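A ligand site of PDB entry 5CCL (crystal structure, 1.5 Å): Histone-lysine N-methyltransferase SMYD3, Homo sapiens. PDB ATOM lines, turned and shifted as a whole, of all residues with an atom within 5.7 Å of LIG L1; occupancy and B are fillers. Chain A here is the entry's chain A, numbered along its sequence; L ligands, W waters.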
ATOM      1  N   CYS A 180     -17.009  31.791 -27.978  1.00  0.00           N
ATOM      2  CA  CYS A 180     -17.077  31.298 -26.626  1.00  0.00           C
ATOM      3  C   CYS A 180     -18.393  30.690 -26.244  1.00  0.00           C
ATOM      4  O   CYS A 180     -18.566  30.386 -25.050  1.00  0.00           O
ATOM      5  CB  CYS A 180     -16.652  32.339 -25.596  1.00  0.00           C
ATOM      6  SG  CYS A 180     -17.692  33.772 -25.660  1.00  0.00           S
ATOM      7  N   ASN A 181     -19.329  30.557 -27.219  1.00  0.00           N
ATOM      8  CA  ASN A 181     -20.620  29.925 -26.935  1.00  0.00           C
ATOM      9  C   ASN A 181     -21.024  28.805 -27.895  1.00  0.00           C
ATOM     10  O   ASN A 181     -22.126  28.332 -27.831  1.00  0.00           O
ATOM     11  CB  ASN A 181     -21.705  30.996 -26.919  1.00  0.00           C
ATOM     12  CG  ASN A 181     -21.517  31.988 -25.786  1.00  0.00           C
ATOM     13  OD1 ASN A 181     -21.781  31.710 -24.601  1.00  0.00           O
ATOM     14  ND2 ASN A 181     -21.040  33.164 -26.128  1.00  0.00           N
ATOM     15  N   SER A 182     -20.115  28.371 -28.754  1.00  0.00           N
ATOM     16  CA  SER A 182     -20.322  27.278 -29.703  1.00  0.00           C
ATOM     17  C   SER A 182     -20.122  25.914 -29.047  1.00  0.00           C
ATOM     18  O   SER A 182     -19.049  25.662 -28.522  1.00  0.00           O
ATOM     19  CB  SER A 182     -19.296  27.364 -30.874  1.00  0.00           C
ATOM     20  OG  SER A 182     -19.667  28.345 -31.819  1.00  0.00           O
ATOM     21  N   PHE A 183     -21.150  25.087 -29.110  1.00  0.00           N
ATOM     22  CA  PHE A 183     -21.100  23.717 -28.592  1.00  0.00           C
ATOM     23  C   PHE A 183     -20.682  22.751 -29.673  1.00  0.00           C
ATOM     24  O   PHE A 183     -21.327  22.718 -30.748  1.00  0.00           O
ATOM     25  CB  PHE A 183     -22.456  23.285 -28.053  1.00  0.00           C
ATOM     26  CG  PHE A 183     -22.841  23.997 -26.792  1.00  0.00           C
ATOM     27  CD1 PHE A 183     -23.436  25.249 -26.816  1.00  0.00           C
ATOM     28  CD2 PHE A 183     -22.629  23.431 -25.559  1.00  0.00           C
ATOM     29  CE1 PHE A 183     -23.806  25.917 -25.670  1.00  0.00           C
ATOM     30  CE2 PHE A 183     -23.016  24.062 -24.407  1.00  0.00           C
ATOM     31  CZ  PHE A 183     -23.591  25.329 -24.447  1.00  0.00           C
ATOM     32  N   THR A 184     -19.707  21.893 -29.373  1.00  0.00           N
ATOM     33  CA  THR A 184     -19.437  20.789 -30.255  1.00  0.00           C
ATOM     34  C   THR A 184     -20.467  19.686 -30.004  1.00  0.00           C
ATOM     35  O   THR A 184     -20.618  19.228 -28.891  1.00  0.00           O
ATOM     36  CB  THR A 184     -18.007  20.267 -30.054  1.00  0.00           C
ATOM     37  OG1 THR A 184     -17.056  21.290 -30.436  1.00  0.00           O
ATOM     38  CG2 THR A 184     -17.745  19.057 -30.878  1.00  0.00           C
ATOM     39  N   ILE A 185     -21.194  19.283 -31.050  1.00  0.00           N
ATOM     40  CA  ILE A 185     -22.228  18.266 -30.978  1.00  0.00           C
ATOM     41  C   ILE A 185     -21.545  16.928 -31.251  1.00  0.00           C
ATOM     42  O   ILE A 185     -20.895  16.793 -32.266  1.00  0.00           O
ATOM     43  CB  ILE A 185     -23.344  18.549 -32.011  1.00  0.00           C
ATOM     44  CG1 ILE A 185     -23.974  19.919 -31.721  1.00  0.00           C
ATOM     45  CG2 ILE A 185     -24.348  17.411 -31.971  1.00  0.00           C
ATOM     46  CD1 ILE A 185     -24.858  20.384 -32.862  1.00  0.00           C
ATOM     47  N   CYS A 186     -21.742  15.956 -30.360  1.00  0.00           N
ATOM     48  CA  CYS A 186     -21.192  14.626 -30.497  1.00  0.00           C
ATOM     49  C   CYS A 186     -22.297  13.630 -30.779  1.00  0.00           C
ATOM     50  O   CYS A 186     -23.422  13.753 -30.284  1.00  0.00           O
ATOM     51  CB  CYS A 186     -20.460  14.242 -29.228  1.00  0.00           C
ATOM     52  SG  CYS A 186     -18.972  15.237 -28.970  1.00  0.00           S
ATOM     53  N   GLU A 192     -17.192  13.735 -32.590  1.00  0.00           N
ATOM     54  CA  GLU A 192     -17.596  15.110 -32.884  1.00  0.00           C
ATOM     55  C   GLU A 192     -18.150  15.151 -34.295  1.00  0.00           C
ATOM     56  O   GLU A 192     -17.504  14.707 -35.232  1.00  0.00           O
ATOM     57  CB  GLU A 192     -16.380  16.052 -32.751  1.00  0.00           C
ATOM     58  CG  GLU A 192     -15.880  16.135 -31.323  1.00  0.00           C
ATOM     59  CD  GLU A 192     -14.701  17.083 -31.087  1.00  0.00           C
ATOM     60  OE1 GLU A 192     -14.267  17.759 -32.045  1.00  0.00           O
ATOM     61  OE2 GLU A 192     -14.257  17.152 -29.923  1.00  0.00           O
ATOM     62  N   ILE A 201     -28.316  27.139 -22.587  1.00  0.00           N
ATOM     63  CA  ILE A 201     -27.269  26.286 -21.995  1.00  0.00           C
ATOM     64  C   ILE A 201     -25.946  27.047 -21.828  1.00  0.00           C
ATOM     65  O   ILE A 201     -25.136  26.702 -20.963  1.00  0.00           O
ATOM     66  CB  ILE A 201     -27.074  24.997 -22.808  1.00  0.00           C
ATOM     67  CG1 ILE A 201     -28.396  24.286 -23.101  1.00  0.00           C
ATOM     68  CG2 ILE A 201     -26.075  24.046 -22.158  1.00  0.00           C
ATOM     69  CD1 ILE A 201     -29.189  23.908 -21.850  1.00  0.00           C
ATOM     70  N   SER A 202     -25.760  28.089 -22.648  1.00  0.00           N
ATOM     71  CA  SER A 202     -24.598  28.940 -22.487  1.00  0.00           C
ATOM     72  C   SER A 202     -24.586  29.723 -21.206  1.00  0.00           C
ATOM     73  O   SER A 202     -23.548  30.325 -20.908  1.00  0.00           O
ATOM     74  CB  SER A 202     -24.439  29.861 -23.665  1.00  0.00           C
ATOM     75  OG  SER A 202     -24.075  29.160 -24.849  1.00  0.00           O
ATOM     76  N   LEU A 204     -24.445  28.302 -18.365  1.00  0.00           N
ATOM     77  CA  LEU A 204     -23.658  27.519 -17.431  1.00  0.00           C
ATOM     78  C   LEU A 204     -22.192  27.897 -17.469  1.00  0.00           C
ATOM     79  O   LEU A 204     -21.551  27.801 -18.514  1.00  0.00           O
ATOM     80  CB  LEU A 204     -23.774  26.029 -17.754  1.00  0.00           C
ATOM     81  CG  LEU A 204     -25.177  25.442 -17.537  1.00  0.00           C
ATOM     82  CD1 LEU A 204     -25.469  24.340 -18.525  1.00  0.00           C
ATOM     83  CD2 LEU A 204     -25.279  24.920 -16.123  1.00  0.00           C
ATOM     84  N   ILE A 214     -23.898  17.840 -20.004  1.00  0.00           N
ATOM     85  CA  ILE A 214     -24.713  17.786 -21.200  1.00  0.00           C
ATOM     86  C   ILE A 214     -24.403  16.585 -22.047  1.00  0.00           C
ATOM     87  O   ILE A 214     -23.285  16.080 -22.067  1.00  0.00           O
ATOM     88  CB  ILE A 214     -24.607  19.085 -22.053  1.00  0.00           C
ATOM     89  CG1 ILE A 214     -23.221  19.253 -22.628  1.00  0.00           C
ATOM     90  CG2 ILE A 214     -25.113  20.265 -21.259  1.00  0.00           C
ATOM     91  CD1 ILE A 214     -23.094  20.429 -23.553  1.00  0.00           C
ATOM     92  N   ILE A 237     -20.790  23.012 -15.926  1.00  0.00           N
ATOM     93  CA  ILE A 237     -20.400  21.917 -16.798  1.00  0.00           C
ATOM     94  C   ILE A 237     -18.941  22.054 -17.132  1.00  0.00           C
ATOM     95  O   ILE A 237     -18.372  23.129 -16.966  1.00  0.00           O
ATOM     96  CB  ILE A 237     -21.294  21.890 -18.079  1.00  0.00           C
ATOM     97  CG1 ILE A 237     -21.191  23.160 -18.919  1.00  0.00           C
ATOM     98  CG2 ILE A 237     -22.725  21.506 -17.719  1.00  0.00           C
ATOM     99  CD1 ILE A 237     -21.987  23.123 -20.224  1.00  0.00           C
ATOM    100  N   CYS A 238     -18.328  20.975 -17.617  1.00  0.00           N
ATOM    101  CA  CYS A 238     -16.924  21.074 -18.018  1.00  0.00           C
ATOM    102  C   CYS A 238     -16.891  21.379 -19.486  1.00  0.00           C
ATOM    103  O   CYS A 238     -17.417  20.622 -20.308  1.00  0.00           O
ATOM    104  CB  CYS A 238     -16.208  19.775 -17.713  1.00  0.00           C
ATOM    105  SG  CYS A 238     -14.435  19.876 -18.021  1.00  0.00           S
ATOM    106  N   TYR A 239     -16.266  22.484 -19.852  1.00  0.00           N
ATOM    107  CA  TYR A 239     -16.165  22.894 -21.260  1.00  0.00           C
ATOM    108  C   TYR A 239     -15.217  22.048 -22.078  1.00  0.00           C
ATOM    109  O   TYR A 239     -15.177  22.140 -23.290  1.00  0.00           O
ATOM    110  CB  TYR A 239     -15.761  24.379 -21.392  1.00  0.00           C
ATOM    111  CG  TYR A 239     -16.716  25.424 -20.860  1.00  0.00           C
ATOM    112  CD1 TYR A 239     -17.899  25.130 -20.248  1.00  0.00           C
ATOM    113  CD2 TYR A 239     -16.368  26.741 -20.949  1.00  0.00           C
ATOM    114  CE1 TYR A 239     -18.740  26.147 -19.785  1.00  0.00           C
ATOM    115  CE2 TYR A 239     -17.157  27.749 -20.478  1.00  0.00           C
ATOM    116  CZ  TYR A 239     -18.366  27.457 -19.890  1.00  0.00           C
ATOM    117  OH  TYR A 239     -19.131  28.500 -19.437  1.00  0.00           O
ATOM    118  N   LEU A 240     -14.402  21.268 -21.379  1.00  0.00           N
ATOM    119  CA  LEU A 240     -13.205  20.665 -21.942  1.00  0.00           C
ATOM    120  C   LEU A 240     -13.151  19.168 -21.904  1.00  0.00           C
ATOM    121  O   LEU A 240     -13.746  18.565 -21.023  1.00  0.00           O
ATOM    122  CB  LEU A 240     -11.969  21.153 -21.162  1.00  0.00           C
ATOM    123  CG  LEU A 240     -11.793  22.640 -20.979  1.00  0.00           C
ATOM    124  CD1 LEU A 240     -10.580  22.915 -20.111  1.00  0.00           C
ATOM    125  CD2 LEU A 240     -11.633  23.278 -22.340  1.00  0.00           C
ATOM    126  N   ASP A 241     -12.381  18.571 -22.803  1.00  0.00           N
ATOM    127  CA  ASP A 241     -11.955  17.138 -22.759  1.00  0.00           C
ATOM    128  C   ASP A 241     -11.307  16.869 -21.413  1.00  0.00           C
ATOM    129  O   ASP A 241     -10.558  17.698 -20.899  1.00  0.00           O
ATOM    130  CB  ASP A 241     -11.019  16.900 -23.976  1.00  0.00           C
ATOM    131  CG  ASP A 241     -10.124  15.604 -23.933  1.00  0.00           C
ATOM    132  OD1 ASP A 241     -10.433  14.497 -23.389  1.00  0.00           O
ATOM    133  OD2 ASP A 241      -9.020  15.738 -24.559  1.00  0.00           O
ATOM    134  N   GLN A 252      -6.519  26.477 -23.186  1.00  0.00           N
ATOM    135  CA  GLN A 252      -7.743  26.511 -23.932  1.00  0.00           C
ATOM    136  C   GLN A 252      -8.744  27.471 -23.302  1.00  0.00           C
ATOM    137  O   GLN A 252      -9.481  28.194 -24.018  1.00  0.00           O
ATOM    138  CB  GLN A 252      -8.352  25.096 -24.102  1.00  0.00           C
ATOM    139  CG  GLN A 252      -9.537  25.065 -25.020  1.00  0.00           C
ATOM    140  CD  GLN A 252     -10.108  23.701 -25.337  1.00  0.00           C
ATOM    141  OE1 GLN A 252      -9.516  22.641 -25.013  1.00  0.00           O
ATOM    142  NE2 GLN A 252     -11.287  23.708 -25.959  1.00  0.00           N
ATOM    143  N   GLN A 256      -9.893  30.423 -25.776  1.00  0.00           N
ATOM    144  CA  GLN A 256     -11.247  30.328 -26.297  1.00  0.00           C
ATOM    145  C   GLN A 256     -12.253  31.088 -25.428  1.00  0.00           C
ATOM    146  O   GLN A 256     -13.252  31.633 -25.946  1.00  0.00           O
ATOM    147  CB  GLN A 256     -11.666  28.840 -26.440  1.00  0.00           C
ATOM    148  CG  GLN A 256     -13.025  28.578 -27.013  1.00  0.00           C
ATOM    149  CD  GLN A 256     -13.198  27.096 -27.363  1.00  0.00           C
ATOM    150  OE1 GLN A 256     -12.263  26.295 -27.189  1.00  0.00           O
ATOM    151  NE2 GLN A 256     -14.365  26.737 -27.836  1.00  0.00           N
ATOM    152  N   TYR A 257     -12.038  31.101 -24.120  1.00  0.00           N
ATOM    153  CA  TYR A 257     -13.059  31.585 -23.163  1.00  0.00           C
ATOM    154  C   TYR A 257     -12.631  32.779 -22.337  1.00  0.00           C
ATOM    155  O   TYR A 257     -13.384  33.299 -21.563  1.00  0.00           O
ATOM    156  CB  TYR A 257     -13.525  30.451 -22.248  1.00  0.00           C
ATOM    157  CG  TYR A 257     -14.162  29.324 -22.993  1.00  0.00           C
ATOM    158  CD1 TYR A 257     -15.468  29.464 -23.434  1.00  0.00           C
ATOM    159  CD2 TYR A 257     -13.481  28.158 -23.295  1.00  0.00           C
ATOM    160  CE1 TYR A 257     -16.082  28.452 -24.098  1.00  0.00           C
ATOM    161  CE2 TYR A 257     -14.105  27.144 -23.997  1.00  0.00           C
ATOM    162  CZ  TYR A 257     -15.404  27.298 -24.379  1.00  0.00           C
ATOM    163  OH  TYR A 257     -16.060  26.281 -25.083  1.00  0.00           O
HETATM  164  O1  LIG L   1     -18.176  21.929 -27.076  1.00  0.00           O
HETATM  165  C1  LIG L   1     -17.836  22.080 -25.889  1.00  0.00           C
HETATM  166  N1  LIG L   1     -16.915  21.232 -25.389  1.00  0.00           N
HETATM  167  C2  LIG L   1     -16.229  20.208 -26.226  1.00  0.00           C
HETATM  168  C3  LIG L   1     -17.111  18.987 -26.388  1.00  0.00           C
HETATM  169  C4  LIG L   1     -16.366  17.918 -27.155  1.00  0.00           C
HETATM  170  N2  LIG L   1     -15.069  17.601 -26.559  1.00  0.00           N
HETATM  171  C5  LIG L   1     -14.201  18.758 -26.441  1.00  0.00           C
HETATM  172  C6  LIG L   1     -14.888  19.843 -25.618  1.00  0.00           C
HETATM  173  C7  LIG L   1     -18.511  23.093 -25.044  1.00  0.00           C
HETATM  174  C8  LIG L   1     -18.897  24.267 -25.695  1.00  0.00           C
HETATM  175  C9  LIG L   1     -19.572  25.246 -24.993  1.00  0.00           C
HETATM  176  C10 LIG L   1     -19.947  24.991 -23.678  1.00  0.00           C
HETATM  177  N3  LIG L   1     -20.650  26.087 -23.192  1.00  0.00           N
HETATM  178  C11 LIG L   1     -20.841  27.052 -24.161  1.00  0.00           C
HETATM  179  O2  LIG L   1     -21.506  28.064 -24.051  1.00  0.00           O
HETATM  180  C12 LIG L   1     -20.132  26.558 -25.400  1.00  0.00           C
HETATM  181  C13 LIG L   1     -19.625  23.822 -22.991  1.00  0.00           C
HETATM  182  C14 LIG L   1     -18.922  22.856 -23.721  1.00  0.00           C
HETATM  183  N1  LG2 L   2     -20.849  33.797 -17.574  1.00  0.00           N
HETATM  184  C1  LG2 L   2     -21.403  33.628 -18.934  1.00  0.00           C
HETATM  185  C2  LG2 L   2     -22.334  34.777 -19.301  1.00  0.00           C
HETATM  186  O1  LG2 L   2     -22.960  34.699 -20.389  1.00  0.00           O
HETATM  187  O2  LG2 L   2     -22.410  35.746 -18.502  1.00  0.00           O
HETATM  188  C3  LG2 L   2     -22.047  32.265 -19.160  1.00  0.00           C
HETATM  189  C4  LG2 L   2     -21.064  31.148 -19.644  1.00  0.00           C
HETATM  190  S1  LG2 L   2     -20.429  31.471 -21.245  1.00  0.00           S
HETATM  191  C5  LG2 L   2     -20.622  30.051 -22.160  1.00  0.00           C
HETATM  192  C6  LG2 L   2     -18.702  31.420 -21.090  1.00  0.00           C
HETATM  193  C7  LG2 L   2     -18.047  32.628 -20.425  1.00  0.00           C
HETATM  194  O3  LG2 L   2     -18.337  32.663 -19.011  1.00  0.00           O
HETATM  195  C8  LG2 L   2     -16.538  32.619 -20.475  1.00  0.00           C
HETATM  196  O4  LG2 L   2     -16.024  33.059 -21.721  1.00  0.00           O
HETATM  197  C9  LG2 L   2     -16.211  33.486 -19.309  1.00  0.00           C
HETATM  198  O5  LG2 L   2     -16.486  34.891 -19.575  1.00  0.00           O
HETATM  199  C10 LG2 L   2     -17.192  33.034 -18.245  1.00  0.00           C
HETATM  200  N2  LG2 L   2     -16.813  31.832 -17.467  1.00  0.00           N
HETATM  201  C11 LG2 L   2     -17.293  30.559 -17.615  1.00  0.00           C
HETATM  202  N3  LG2 L   2     -16.817  29.778 -16.624  1.00  0.00           N
HETATM  203  C12 LG2 L   2     -16.008  30.571 -15.834  1.00  0.00           C
HETATM  204  C13 LG2 L   2     -15.240  30.315 -14.653  1.00  0.00           C
HETATM  205  N4  LG2 L   2     -15.191  29.102 -14.101  1.00  0.00           N
HETATM  206  N5  LG2 L   2     -14.539  31.349 -14.126  1.00  0.00           N
HETATM  207  C14 LG2 L   2     -14.611  32.552 -14.723  1.00  0.00           C
HETATM  208  N6  LG2 L   2     -15.337  32.900 -15.805  1.00  0.00           N
HETATM  209  C15 LG2 L   2     -16.040  31.904 -16.375  1.00  0.00           C
HETATM  210  O   HOH W   1     -22.240  26.626 -20.947  1.00  0.00           O
HETATM  211  O   HOH W   2     -19.896  20.342 -21.548  1.00  0.00           O
HETATM  212  O   HOH W   3     -20.663  20.430 -26.428  1.00  0.00           O
HETATM  213  O   HOH W   4     -14.769  23.973 -25.350  1.00  0.00           O
HETATM  214  O   HOH W   5     -17.110  19.254 -22.715  1.00  0.00           O
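The side-chain hydroxyl (OG) of Ser 202 sits at hydrogen-bond distance from an oxygen (O2) of LIG L1, 2.9 Å away. An oxygen (O1) of LIG L1 is in hydrogen-bond range of the backbone NH (N) of Thr 184 (2.8 Å). An oxygen (O4) of LG2 L2 lies within hydrogen-bond range of the backbone carbonyl oxygen (O) of Tyr 257 (2.7 Å). O of Tyr 239 lies within hydrogen-bond range of N1 of LIG L1 (2.9 Å). The side-chain carboxylate (OE2) of Glu 192 is in salt-bridge range of a nitrogen (N2) of LIG L1 (3.5 Å).
The backbone carbonyl oxygen (O) of Leu 204 sits at hydrogen-bond distance from the side-chain hydroxyl (OH) of Tyr 239, 2.7 Å away. The side-chain amide nitrogen (ND2) of Asn 181 sits at hydrogen-bond distance from the side-chain sulfur (SG) of Cys 180, at 3.4 Å. The side-chain hydroxyl (OH) of Tyr 257 is in hydrogen-bond range of the side-chain amide nitrogen (NE2) of Gln 256. OD1 of Asn 181 sits close to OG of Ser 202, 3.4 Å away.
Residues that only touch LIG L1: Ser 182 (3.2 Å), Phe 183 (3.3 Å), Asn 181 (3.5 Å), Tyr 257 (3.5 Å), Ile 237 (3.7 Å), Cys 180 (3.9 Å) and Asp 241 (3.98 Å). Hydrophobic or aromatic side chains that line LIG L1: Phe 183, Ile 237 and Tyr 239. The nearest printed residue that does not touch LIG L1 is Leu 240 (4.1 Å).
Water W1 lies within hydrogen-bond range of O of Leu 204, N3 of LIG L1 and O of Ile 201. Water W3 lies within hydrogen-bond range of O of Thr 184 (2.7 Å) and O1 of LIG L1 (3.0 Å). Water W5 lies within hydrogen-bond range of O of Cys 238 and N1 of LIG L1. Water W4 lies within hydrogen-bond range of the side-chain hydroxyl of Tyr 257 (2.7 Å), the backbone carbonyl oxygen of Tyr 239 (2.8 Å) and a nitrogen (N1) of LIG L1 (3.5 Å).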
